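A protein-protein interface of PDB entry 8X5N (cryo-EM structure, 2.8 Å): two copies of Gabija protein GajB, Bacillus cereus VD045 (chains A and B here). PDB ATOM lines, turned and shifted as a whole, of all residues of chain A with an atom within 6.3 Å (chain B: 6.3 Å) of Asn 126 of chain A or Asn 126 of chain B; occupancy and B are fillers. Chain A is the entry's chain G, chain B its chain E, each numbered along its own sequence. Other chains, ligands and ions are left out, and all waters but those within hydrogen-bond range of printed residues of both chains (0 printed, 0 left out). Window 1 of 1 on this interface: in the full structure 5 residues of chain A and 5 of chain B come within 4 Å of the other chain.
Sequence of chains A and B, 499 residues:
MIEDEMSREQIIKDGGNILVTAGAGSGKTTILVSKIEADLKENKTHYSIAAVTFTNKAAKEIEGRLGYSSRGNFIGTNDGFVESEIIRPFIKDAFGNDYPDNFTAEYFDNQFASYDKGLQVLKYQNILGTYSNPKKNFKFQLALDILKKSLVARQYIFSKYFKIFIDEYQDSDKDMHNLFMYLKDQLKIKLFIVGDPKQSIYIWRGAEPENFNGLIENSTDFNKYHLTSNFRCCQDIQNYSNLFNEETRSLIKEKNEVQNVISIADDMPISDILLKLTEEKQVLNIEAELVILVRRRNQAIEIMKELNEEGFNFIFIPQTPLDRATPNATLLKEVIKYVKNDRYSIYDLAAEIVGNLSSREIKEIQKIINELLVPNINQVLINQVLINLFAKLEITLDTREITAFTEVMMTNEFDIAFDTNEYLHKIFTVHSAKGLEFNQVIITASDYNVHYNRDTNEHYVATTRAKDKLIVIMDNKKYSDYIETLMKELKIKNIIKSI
O of Gln 125 of chain B sits close to OD1 of Asn 126 of chain A (3.0 Å).
The backbone carbonyl oxygen of Gln 125 of chain B sits close to the backbone carbonyl oxygen of Gln 125 of chain A (3.0 Å).
Printed residues of chain B that touch a printed residue of chain A: Asn 102, Thr 104, Tyr 124, Gln 125 and Asn 126.
Among the printed residues, no Asp or Glu carboxylate lies within 4 Å of a Lys or Arg side-chain nitrogen of the other chain.
Thr 104 of chain A touches Asn 126 of chain B, and with the chains exchanged Asn 126 of chain A touches Thr 104 of chain B.
Gln 125 of chain B touches its own counterpart, Gln 125 of chain A.
Asn 126 of chain A touches its own counterpart, Asn 126 of chain B.
Ile 127 of chain A touches Tyr 124 of chain B, but with the chains exchanged Tyr 124 of chain A does not touch Ile 127 of chain B (4.9 Å).
Of the 7 pairs that touch across the chains among the printed residues, 5 have their exchanged pair printed and touching as well.
Of chain B, only Thr 104 (3.9 Å), Gln 125 (3.0 Å) and Asn 126 (3.4 Å) come within 4 Å of Asn 126 of chain A.
Of chain A, only Thr 104 and Asn 126 come within 4 Å of Asn 126 of chain B.
Of the printed residues of chain A, Asn 102 of chain B touches Asn 102 (3.7 Å).
Of the printed residues of chain A, Gln 125 of chain B touches Gln 125 (3.0 Å) and Asn 126 (3.0 Å).
Of the printed residues of chain B, Thr 104 of chain A touches Asn 126 (3.9 Å).
Of the printed residues of chain B, Ile 127 of chain A touches Tyr 124 (3.7 Å).
Phe 103 of chain B touches none of the printed residues of chain A.
The backbone carbonyl oxygen (O) of Asn 102 of chain B lies close to the side-chain amide oxygen (OD1) of Asn 126 of chain B (3.0 Å).
N of Leu 128 of chain A sits at hydrogen-bond distance from O of Thr 104 of chain A, at 3.3 Å.
O of Gln 120 of chain A sits close to OE1 of Gln 125 of chain A (3.3 Å).
The backbone carbonyl oxygen (O) of Val 121 of chain A sits at hydrogen-bond distance from the backbone NH (N) of Asn 126 of chain A (2.9 Å).
N of Ile 127 of chain A lies within hydrogen-bond range of O of Val 121 of chain A (3.5 Å).
ND2 of Asn 102 of chain A touches ND2 of Asn 102 of chain B (3.7 Å).
OG1 of Thr 104 of chain A touches ND2 of Asn 126 of chain B, at 3.9 Å.
ND2 of Asn 126 of chain A touches OG1 of Thr 104 of chain B (3.9 Å).
Asn 126 of chain A touches Asn 126 of chain B (OD1 to CB, 3.4 Å).
Tyr 124 of chain B touches Ile 127 of chain A (O to CG1, 3.7 Å).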
ATOM      1  N   PRO A 100     -23.383 -17.478  -3.667  1.00  0.00           N
ATOM      2  CA  PRO A 100     -23.261 -16.017  -3.663  1.00  0.00           C
ATOM      3  C   PRO A 100     -24.151 -15.324  -4.683  1.00  0.00           C
ATOM      4  O   PRO A 100     -24.415 -15.824  -5.778  1.00  0.00           O
ATOM      5  CB  PRO A 100     -21.779 -15.796  -3.998  1.00  0.00           C
ATOM      6  CG  PRO A 100     -21.401 -16.964  -4.824  1.00  0.00           C
ATOM      7  CD  PRO A 100     -22.279 -18.114  -4.417  1.00  0.00           C
ATOM      8  N   ASN A 102     -23.402 -12.016  -5.693  1.00  0.00           N
ATOM      9  CA  ASN A 102     -22.490 -11.269  -6.546  1.00  0.00           C
ATOM     10  C   ASN A 102     -21.331 -12.137  -7.037  1.00  0.00           C
ATOM     11  O   ASN A 102     -20.732 -12.902  -6.275  1.00  0.00           O
ATOM     12  CB  ASN A 102     -22.031  -9.962  -5.868  1.00  0.00           C
ATOM     13  CG  ASN A 102     -21.390 -10.141  -4.476  1.00  0.00           C
ATOM     14  OD1 ASN A 102     -21.192 -11.237  -3.963  1.00  0.00           O
ATOM     15  ND2 ASN A 102     -21.060  -9.012  -3.865  1.00  0.00           N
ATOM     16  N   PHE A 103     -21.083 -12.066  -8.342  1.00  0.00           N
ATOM     17  CA  PHE A 103     -20.082 -12.889  -9.004  1.00  0.00           C
ATOM     18  C   PHE A 103     -19.655 -12.176 -10.277  1.00  0.00           C
ATOM     19  O   PHE A 103     -20.392 -11.353 -10.827  1.00  0.00           O
ATOM     20  CB  PHE A 103     -20.583 -14.328  -9.284  1.00  0.00           C
ATOM     21  CG  PHE A 103     -21.863 -14.426 -10.094  1.00  0.00           C
ATOM     22  CD1 PHE A 103     -23.115 -14.416  -9.460  1.00  0.00           C
ATOM     23  CD2 PHE A 103     -21.810 -14.611 -11.479  1.00  0.00           C
ATOM     24  CE1 PHE A 103     -24.292 -14.527 -10.201  1.00  0.00           C
ATOM     25  CE2 PHE A 103     -22.979 -14.727 -12.228  1.00  0.00           C
ATOM     26  CZ  PHE A 103     -24.218 -14.683 -11.586  1.00  0.00           C
ATOM     27  N   THR A 104     -18.452 -12.501 -10.736  1.00  0.00           N
ATOM     28  CA  THR A 104     -17.877 -11.907 -11.934  1.00  0.00           C
ATOM     29  C   THR A 104     -18.009 -12.906 -13.074  1.00  0.00           C
ATOM     30  O   THR A 104     -17.564 -14.052 -12.954  1.00  0.00           O
ATOM     31  CB  THR A 104     -16.413 -11.525 -11.709  1.00  0.00           C
ATOM     32  OG1 THR A 104     -16.313 -10.673 -10.560  1.00  0.00           O
ATOM     33  CG2 THR A 104     -15.855 -10.791 -12.919  1.00  0.00           C
ATOM     34  N   GLN A 120     -18.887 -25.957  -8.092  1.00  0.00           N
ATOM     35  CA  GLN A 120     -17.890 -25.708  -7.052  1.00  0.00           C
ATOM     36  C   GLN A 120     -17.051 -24.465  -7.339  1.00  0.00           C
ATOM     37  O   GLN A 120     -16.633 -23.780  -6.397  1.00  0.00           O
ATOM     38  CB  GLN A 120     -16.986 -26.929  -6.895  1.00  0.00           C
ATOM     39  CG  GLN A 120     -17.596 -28.048  -6.069  1.00  0.00           C
ATOM     40  CD  GLN A 120     -16.551 -28.872  -5.345  1.00  0.00           C
ATOM     41  OE1 GLN A 120     -16.754 -29.292  -4.207  1.00  0.00           O
ATOM     42  NE2 GLN A 120     -15.424 -29.109  -6.006  1.00  0.00           N
ATOM     43  N   VAL A 121     -16.785 -24.177  -8.618  1.00  0.00           N
ATOM     44  CA  VAL A 121     -16.124 -22.928  -9.006  1.00  0.00           C
ATOM     45  C   VAL A 121     -17.049 -21.733  -8.761  1.00  0.00           C
ATOM     46  O   VAL A 121     -16.614 -20.690  -8.248  1.00  0.00           O
ATOM     47  CB  VAL A 121     -15.633 -23.040 -10.470  1.00  0.00           C
ATOM     48  CG1 VAL A 121     -15.262 -21.697 -11.101  1.00  0.00           C
ATOM     49  CG2 VAL A 121     -14.402 -23.929 -10.527  1.00  0.00           C
ATOM     50  N   LEU A 122     -18.352 -21.902  -9.037  1.00  0.00           N
ATOM     51  CA  LEU A 122     -19.334 -20.845  -8.788  1.00  0.00           C
ATOM     52  C   LEU A 122     -19.597 -20.624  -7.294  1.00  0.00           C
ATOM     53  O   LEU A 122     -19.904 -19.500  -6.885  1.00  0.00           O
ATOM     54  CB  LEU A 122     -20.636 -21.182  -9.527  1.00  0.00           C
ATOM     55  CG  LEU A 122     -21.830 -20.226  -9.664  1.00  0.00           C
ATOM     56  CD1 LEU A 122     -22.467 -20.492 -10.993  1.00  0.00           C
ATOM     57  CD2 LEU A 122     -22.900 -20.421  -8.602  1.00  0.00           C
ATOM     58  N   LYS A 123     -19.492 -21.668  -6.477  1.00  0.00           N
ATOM     59  CA  LYS A 123     -19.779 -21.550  -5.053  1.00  0.00           C
ATOM     60  C   LYS A 123     -18.555 -21.126  -4.249  1.00  0.00           C
ATOM     61  O   LYS A 123     -18.620 -20.166  -3.475  1.00  0.00           O
ATOM     62  CB  LYS A 123     -20.327 -22.878  -4.526  1.00  0.00           C
ATOM     63  CG  LYS A 123     -20.570 -22.905  -3.029  1.00  0.00           C
ATOM     64  CD  LYS A 123     -21.438 -24.088  -2.646  1.00  0.00           C
ATOM     65  CE  LYS A 123     -20.720 -25.403  -2.891  1.00  0.00           C
ATOM     66  NZ  LYS A 123     -21.507 -26.563  -2.389  1.00  0.00           N
ATOM     67  N   TYR A 124     -17.433 -21.825  -4.421  1.00  0.00           N
ATOM     68  CA  TYR A 124     -16.232 -21.569  -3.638  1.00  0.00           C
ATOM     69  C   TYR A 124     -15.418 -20.407  -4.193  1.00  0.00           C
ATOM     70  O   TYR A 124     -15.079 -19.474  -3.459  1.00  0.00           O
ATOM     71  CB  TYR A 124     -15.369 -22.833  -3.586  1.00  0.00           C
ATOM     72  CG  TYR A 124     -16.012 -23.989  -2.858  1.00  0.00           C
ATOM     73  CD1 TYR A 124     -16.809 -23.772  -1.727  1.00  0.00           C
ATOM     74  CD2 TYR A 124     -15.831 -25.303  -3.310  1.00  0.00           C
ATOM     75  CE1 TYR A 124     -17.407 -24.838  -1.055  1.00  0.00           C
ATOM     76  CE2 TYR A 124     -16.423 -26.378  -2.647  1.00  0.00           C
ATOM     77  CZ  TYR A 124     -17.208 -26.133  -1.524  1.00  0.00           C
ATOM     78  OH  TYR A 124     -17.793 -27.191  -0.869  1.00  0.00           O
ATOM     79  N   GLN A 125     -15.100 -20.449  -5.484  1.00  0.00           N
ATOM     80  CA  GLN A 125     -14.203 -19.485  -6.102  1.00  0.00           C
ATOM     81  C   GLN A 125     -14.936 -18.365  -6.831  1.00  0.00           C
ATOM     82  O   GLN A 125     -14.285 -17.624  -7.572  1.00  0.00           O
ATOM     83  CB  GLN A 125     -13.255 -20.194  -7.073  1.00  0.00           C
ATOM     84  CG  GLN A 125     -12.161 -21.013  -6.407  1.00  0.00           C
ATOM     85  CD  GLN A 125     -12.545 -22.466  -6.218  1.00  0.00           C
ATOM     86  OE1 GLN A 125     -13.513 -22.945  -6.807  1.00  0.00           O
ATOM     87  NE2 GLN A 125     -11.783 -23.178  -5.397  1.00  0.00           N
ATOM     88  N   ASN A 126     -16.276 -18.307  -6.701  1.00  0.00           N
ATOM     89  CA  ASN A 126     -17.295 -17.327  -7.134  1.00  0.00           C
ATOM     90  C   ASN A 126     -17.101 -16.659  -8.510  1.00  0.00           C
ATOM     91  O   ASN A 126     -17.491 -15.509  -8.739  1.00  0.00           O
ATOM     92  CB  ASN A 126     -17.573 -16.316  -5.978  1.00  0.00           C
ATOM     93  CG  ASN A 126     -16.525 -15.197  -5.790  1.00  0.00           C
ATOM     94  OD1 ASN A 126     -15.373 -15.296  -6.182  1.00  0.00           O
ATOM     95  ND2 ASN A 126     -16.970 -14.105  -5.181  1.00  0.00           N
ATOM     96  N   ILE A 127     -16.596 -17.429  -9.469  1.00  0.00           N
ATOM     97  CA  ILE A 127     -16.489 -17.013 -10.863  1.00  0.00           C
ATOM     98  C   ILE A 127     -17.446 -17.883 -11.670  1.00  0.00           C
ATOM     99  O   ILE A 127     -17.447 -19.112 -11.520  1.00  0.00           O
ATOM    100  CB  ILE A 127     -15.036 -17.127 -11.370  1.00  0.00           C
ATOM    101  CG1 ILE A 127     -14.120 -16.176 -10.596  1.00  0.00           C
ATOM    102  CG2 ILE A 127     -14.914 -16.831 -12.864  1.00  0.00           C
ATOM    103  CD1 ILE A 127     -14.495 -14.711 -10.716  1.00  0.00           C
ATOM    104  N   LEU A 128     -18.291 -17.243 -12.482  1.00  0.00           N
ATOM    105  CA  LEU A 128     -19.250 -17.929 -13.348  1.00  0.00           C
ATOM    106  C   LEU A 128     -18.495 -18.637 -14.466  1.00  0.00           C
ATOM    107  O   LEU A 128     -18.074 -18.017 -15.445  1.00  0.00           O
ATOM    108  CB  LEU A 128     -20.257 -16.930 -13.905  1.00  0.00           C
ATOM    109  CG  LEU A 128     -21.367 -17.430 -14.830  1.00  0.00           C
ATOM    110  CD1 LEU A 128     -22.362 -18.293 -14.087  1.00  0.00           C
ATOM    111  CD2 LEU A 128     -22.066 -16.251 -15.476  1.00  0.00           C
ATOM    112  N   PRO B 100     -10.672  -7.070  -8.656  1.00  0.00           N
ATOM    113  CA  PRO B 100     -12.110  -6.794  -8.522  1.00  0.00           C
ATOM    114  C   PRO B 100     -12.430  -5.854  -7.367  1.00  0.00           C
ATOM    115  O   PRO B 100     -11.742  -5.829  -6.342  1.00  0.00           O
ATOM    116  CB  PRO B 100     -12.721  -8.181  -8.281  1.00  0.00           C
ATOM    117  CG  PRO B 100     -11.702  -9.144  -8.775  1.00  0.00           C
ATOM    118  CD  PRO B 100     -10.393  -8.504  -8.448  1.00  0.00           C
ATOM    119  N   ASP B 101     -13.494  -5.068  -7.565  1.00  0.00           N
ATOM    120  CA  ASP B 101     -13.893  -4.051  -6.596  1.00  0.00           C
ATOM    121  C   ASP B 101     -14.529  -4.678  -5.361  1.00  0.00           C
ATOM    122  O   ASP B 101     -14.204  -4.312  -4.227  1.00  0.00           O
ATOM    123  CB  ASP B 101     -14.865  -3.069  -7.252  1.00  0.00           C
ATOM    124  CG  ASP B 101     -14.661  -1.644  -6.787  1.00  0.00           C
ATOM    125  OD1 ASP B 101     -13.753  -1.408  -5.968  1.00  0.00           O
ATOM    126  OD2 ASP B 101     -15.413  -0.757  -7.241  1.00  0.00           O
ATOM    127  N   ASN B 102     -15.433  -5.629  -5.565  1.00  0.00           N
ATOM    128  CA  ASN B 102     -16.070  -6.352  -4.476  1.00  0.00           C
ATOM    129  C   ASN B 102     -15.401  -7.708  -4.273  1.00  0.00           C
ATOM    130  O   ASN B 102     -14.765  -8.264  -5.171  1.00  0.00           O
ATOM    131  CB  ASN B 102     -17.574  -6.511  -4.738  1.00  0.00           C
ATOM    132  CG  ASN B 102     -17.891  -6.999  -6.150  1.00  0.00           C
ATOM    133  OD1 ASN B 102     -17.001  -7.230  -6.969  1.00  0.00           O
ATOM    134  ND2 ASN B 102     -19.178  -7.158  -6.433  1.00  0.00           N
ATOM    135  N   PHE B 103     -15.564  -8.243  -3.069  1.00  0.00           N
ATOM    136  CA  PHE B 103     -14.948  -9.506  -2.689  1.00  0.00           C
ATOM    137  C   PHE B 103     -15.870 -10.190  -1.686  1.00  0.00           C
ATOM    138  O   PHE B 103     -17.030  -9.801  -1.518  1.00  0.00           O
ATOM    139  CB  PHE B 103     -13.535  -9.289  -2.127  1.00  0.00           C
ATOM    140  CG  PHE B 103     -13.375  -8.026  -1.309  1.00  0.00           C
ATOM    141  CD1 PHE B 103     -13.813  -7.978   0.021  1.00  0.00           C
ATOM    142  CD2 PHE B 103     -12.755  -6.900  -1.859  1.00  0.00           C
ATOM    143  CE1 PHE B 103     -13.665  -6.821   0.780  1.00  0.00           C
ATOM    144  CE2 PHE B 103     -12.599  -5.734  -1.106  1.00  0.00           C
ATOM    145  CZ  PHE B 103     -13.056  -5.701   0.216  1.00  0.00           C
ATOM    146  N   THR B 104     -15.350 -11.218  -1.023  1.00  0.00           N
ATOM    147  CA  THR B 104     -16.043 -11.871   0.078  1.00  0.00           C
ATOM    148  C   THR B 104     -15.024 -12.125   1.179  1.00  0.00           C
ATOM    149  O   THR B 104     -13.940 -12.648   0.908  1.00  0.00           O
ATOM    150  CB  THR B 104     -16.702 -13.183  -0.376  1.00  0.00           C
ATOM    151  OG1 THR B 104     -17.523 -12.934  -1.524  1.00  0.00           O
ATOM    152  CG2 THR B 104     -17.581 -13.760   0.723  1.00  0.00           C
ATOM    153  N   VAL B 121      -4.196 -15.241  -5.441  1.00  0.00           N
ATOM    154  CA  VAL B 121      -5.497 -15.601  -4.860  1.00  0.00           C
ATOM    155  C   VAL B 121      -6.486 -14.439  -4.978  1.00  0.00           C
ATOM    156  O   VAL B 121      -7.648 -14.632  -5.369  1.00  0.00           O
ATOM    157  CB  VAL B 121      -5.318 -16.084  -3.398  1.00  0.00           C
ATOM    158  CG1 VAL B 121      -6.639 -16.351  -2.706  1.00  0.00           C
ATOM    159  CG2 VAL B 121      -4.602 -17.417  -3.377  1.00  0.00           C
ATOM    160  N   LEU B 122      -6.018 -13.211  -4.708  1.00  0.00           N
ATOM    161  CA  LEU B 122      -6.856 -12.013  -4.809  1.00  0.00           C
ATOM    162  C   LEU B 122      -7.214 -11.662  -6.256  1.00  0.00           C
ATOM    163  O   LEU B 122      -8.295 -11.111  -6.508  1.00  0.00           O
ATOM    164  CB  LEU B 122      -6.141 -10.833  -4.145  1.00  0.00           C
ATOM    165  CG  LEU B 122      -6.900  -9.528  -3.885  1.00  0.00           C
ATOM    166  CD1 LEU B 122      -8.201  -9.776  -3.137  1.00  0.00           C
ATOM    167  CD2 LEU B 122      -6.023  -8.536  -3.153  1.00  0.00           C
ATOM    168  N   LYS B 123      -6.353 -12.012  -7.215  1.00  0.00           N
ATOM    169  CA  LYS B 123      -6.586 -11.645  -8.609  1.00  0.00           C
ATOM    170  C   LYS B 123      -7.642 -12.526  -9.269  1.00  0.00           C
ATOM    171  O   LYS B 123      -8.575 -12.021  -9.903  1.00  0.00           O
ATOM    172  CB  LYS B 123      -5.275 -11.713  -9.395  1.00  0.00           C
ATOM    173  CG  LYS B 123      -5.356 -11.067 -10.768  1.00  0.00           C
ATOM    174  CD  LYS B 123      -3.974 -10.797 -11.340  1.00  0.00           C
ATOM    175  CE  LYS B 123      -4.016 -10.725 -12.858  1.00  0.00           C
ATOM    176  NZ  LYS B 123      -2.776 -10.131 -13.427  1.00  0.00           N
ATOM    177  N   TYR B 124      -7.521 -13.845  -9.124  1.00  0.00           N
ATOM    178  CA  TYR B 124      -8.320 -14.757  -9.937  1.00  0.00           C
ATOM    179  C   TYR B 124      -9.648 -15.135  -9.282  1.00  0.00           C
ATOM    180  O   TYR B 124     -10.714 -14.897  -9.857  1.00  0.00           O
ATOM    181  CB  TYR B 124      -7.503 -16.013 -10.264  1.00  0.00           C
ATOM    182  CG  TYR B 124      -6.243 -15.729 -11.054  1.00  0.00           C
ATOM    183  CD1 TYR B 124      -6.281 -14.909 -12.189  1.00  0.00           C
ATOM    184  CD2 TYR B 124      -5.020 -16.296 -10.677  1.00  0.00           C
ATOM    185  CE1 TYR B 124      -5.122 -14.645 -12.925  1.00  0.00           C
ATOM    186  CE2 TYR B 124      -3.853 -16.040 -11.403  1.00  0.00           C
ATOM    187  CZ  TYR B 124      -3.917 -15.217 -12.522  1.00  0.00           C
ATOM    188  OH  TYR B 124      -2.771 -14.964 -13.240  1.00  0.00           O
ATOM    189  N   GLN B 125      -9.604 -15.727  -8.089  1.00  0.00           N
ATOM    190  CA  GLN B 125     -10.781 -16.370  -7.517  1.00  0.00           C
ATOM    191  C   GLN B 125     -11.524 -15.517  -6.491  1.00  0.00           C
ATOM    192  O   GLN B 125     -12.466 -16.031  -5.874  1.00  0.00           O
ATOM    193  CB  GLN B 125     -10.402 -17.718  -6.897  1.00  0.00           C
ATOM    194  CG  GLN B 125      -9.353 -17.664  -5.810  1.00  0.00           C
ATOM    195  CD  GLN B 125      -7.991 -18.103  -6.305  1.00  0.00           C
ATOM    196  OE1 GLN B 125      -7.678 -17.983  -7.489  1.00  0.00           O
ATOM    197  NE2 GLN B 125      -7.176 -18.629  -5.399  1.00  0.00           N
ATOM    198  N   ASN B 126     -11.089 -14.262  -6.278  1.00  0.00           N
ATOM    199  CA  ASN B 126     -11.842 -13.161  -5.639  1.00  0.00           C
ATOM    200  C   ASN B 126     -12.198 -13.435  -4.172  1.00  0.00           C
ATOM    201  O   ASN B 126     -13.354 -13.338  -3.757  1.00  0.00           O
ATOM    202  CB  ASN B 126     -13.099 -12.820  -6.454  1.00  0.00           C
ATOM    203  CG  ASN B 126     -13.507 -11.366  -6.326  1.00  0.00           C
ATOM    204  OD1 ASN B 126     -12.949 -10.619  -5.524  1.00  0.00           O
ATOM    205  ND2 ASN B 126     -14.491 -10.958  -7.119  1.00  0.00           N
ATOM    206  N   ILE B 127     -11.181 -13.781  -3.387  1.00  0.00           N
ATOM    207  CA  ILE B 127     -11.388 -14.125  -1.984  1.00  0.00           C
ATOM    208  C   ILE B 127     -10.188 -13.593  -1.196  1.00  0.00           C
ATOM    209  O   ILE B 127      -9.096 -13.419  -1.747  1.00  0.00           O
ATOM    210  CB  ILE B 127     -11.634 -15.653  -1.834  1.00  0.00           C
ATOM    211  CG1 ILE B 127     -12.323 -16.015  -0.515  1.00  0.00           C
ATOM    212  CG2 ILE B 127     -10.374 -16.491  -2.040  1.00  0.00           C
ATOM    213  CD1 ILE B 127     -13.798 -15.712  -0.516  1.00  0.00           C
ATOM    214  N   LEU B 128     -10.414 -13.251   0.074  1.00  0.00           N
ATOM    215  CA  LEU B 128      -9.376 -12.699   0.947  1.00  0.00           C
ATOM    216  C   LEU B 128      -8.968 -13.763   1.960  1.00  0.00           C
ATOM    217  O   LEU B 128      -9.658 -13.982   2.958  1.00  0.00           O
ATOM    218  CB  LEU B 128      -9.866 -11.437   1.651  1.00  0.00           C
ATOM    219  CG  LEU B 128      -9.801 -10.109   0.899  1.00  0.00           C
ATOM    220  CD1 LEU B 128     -10.539  -9.035   1.673  1.00  0.00           C
ATOM    221  CD2 LEU B 128      -8.353  -9.701   0.688  1.00  0.00           C
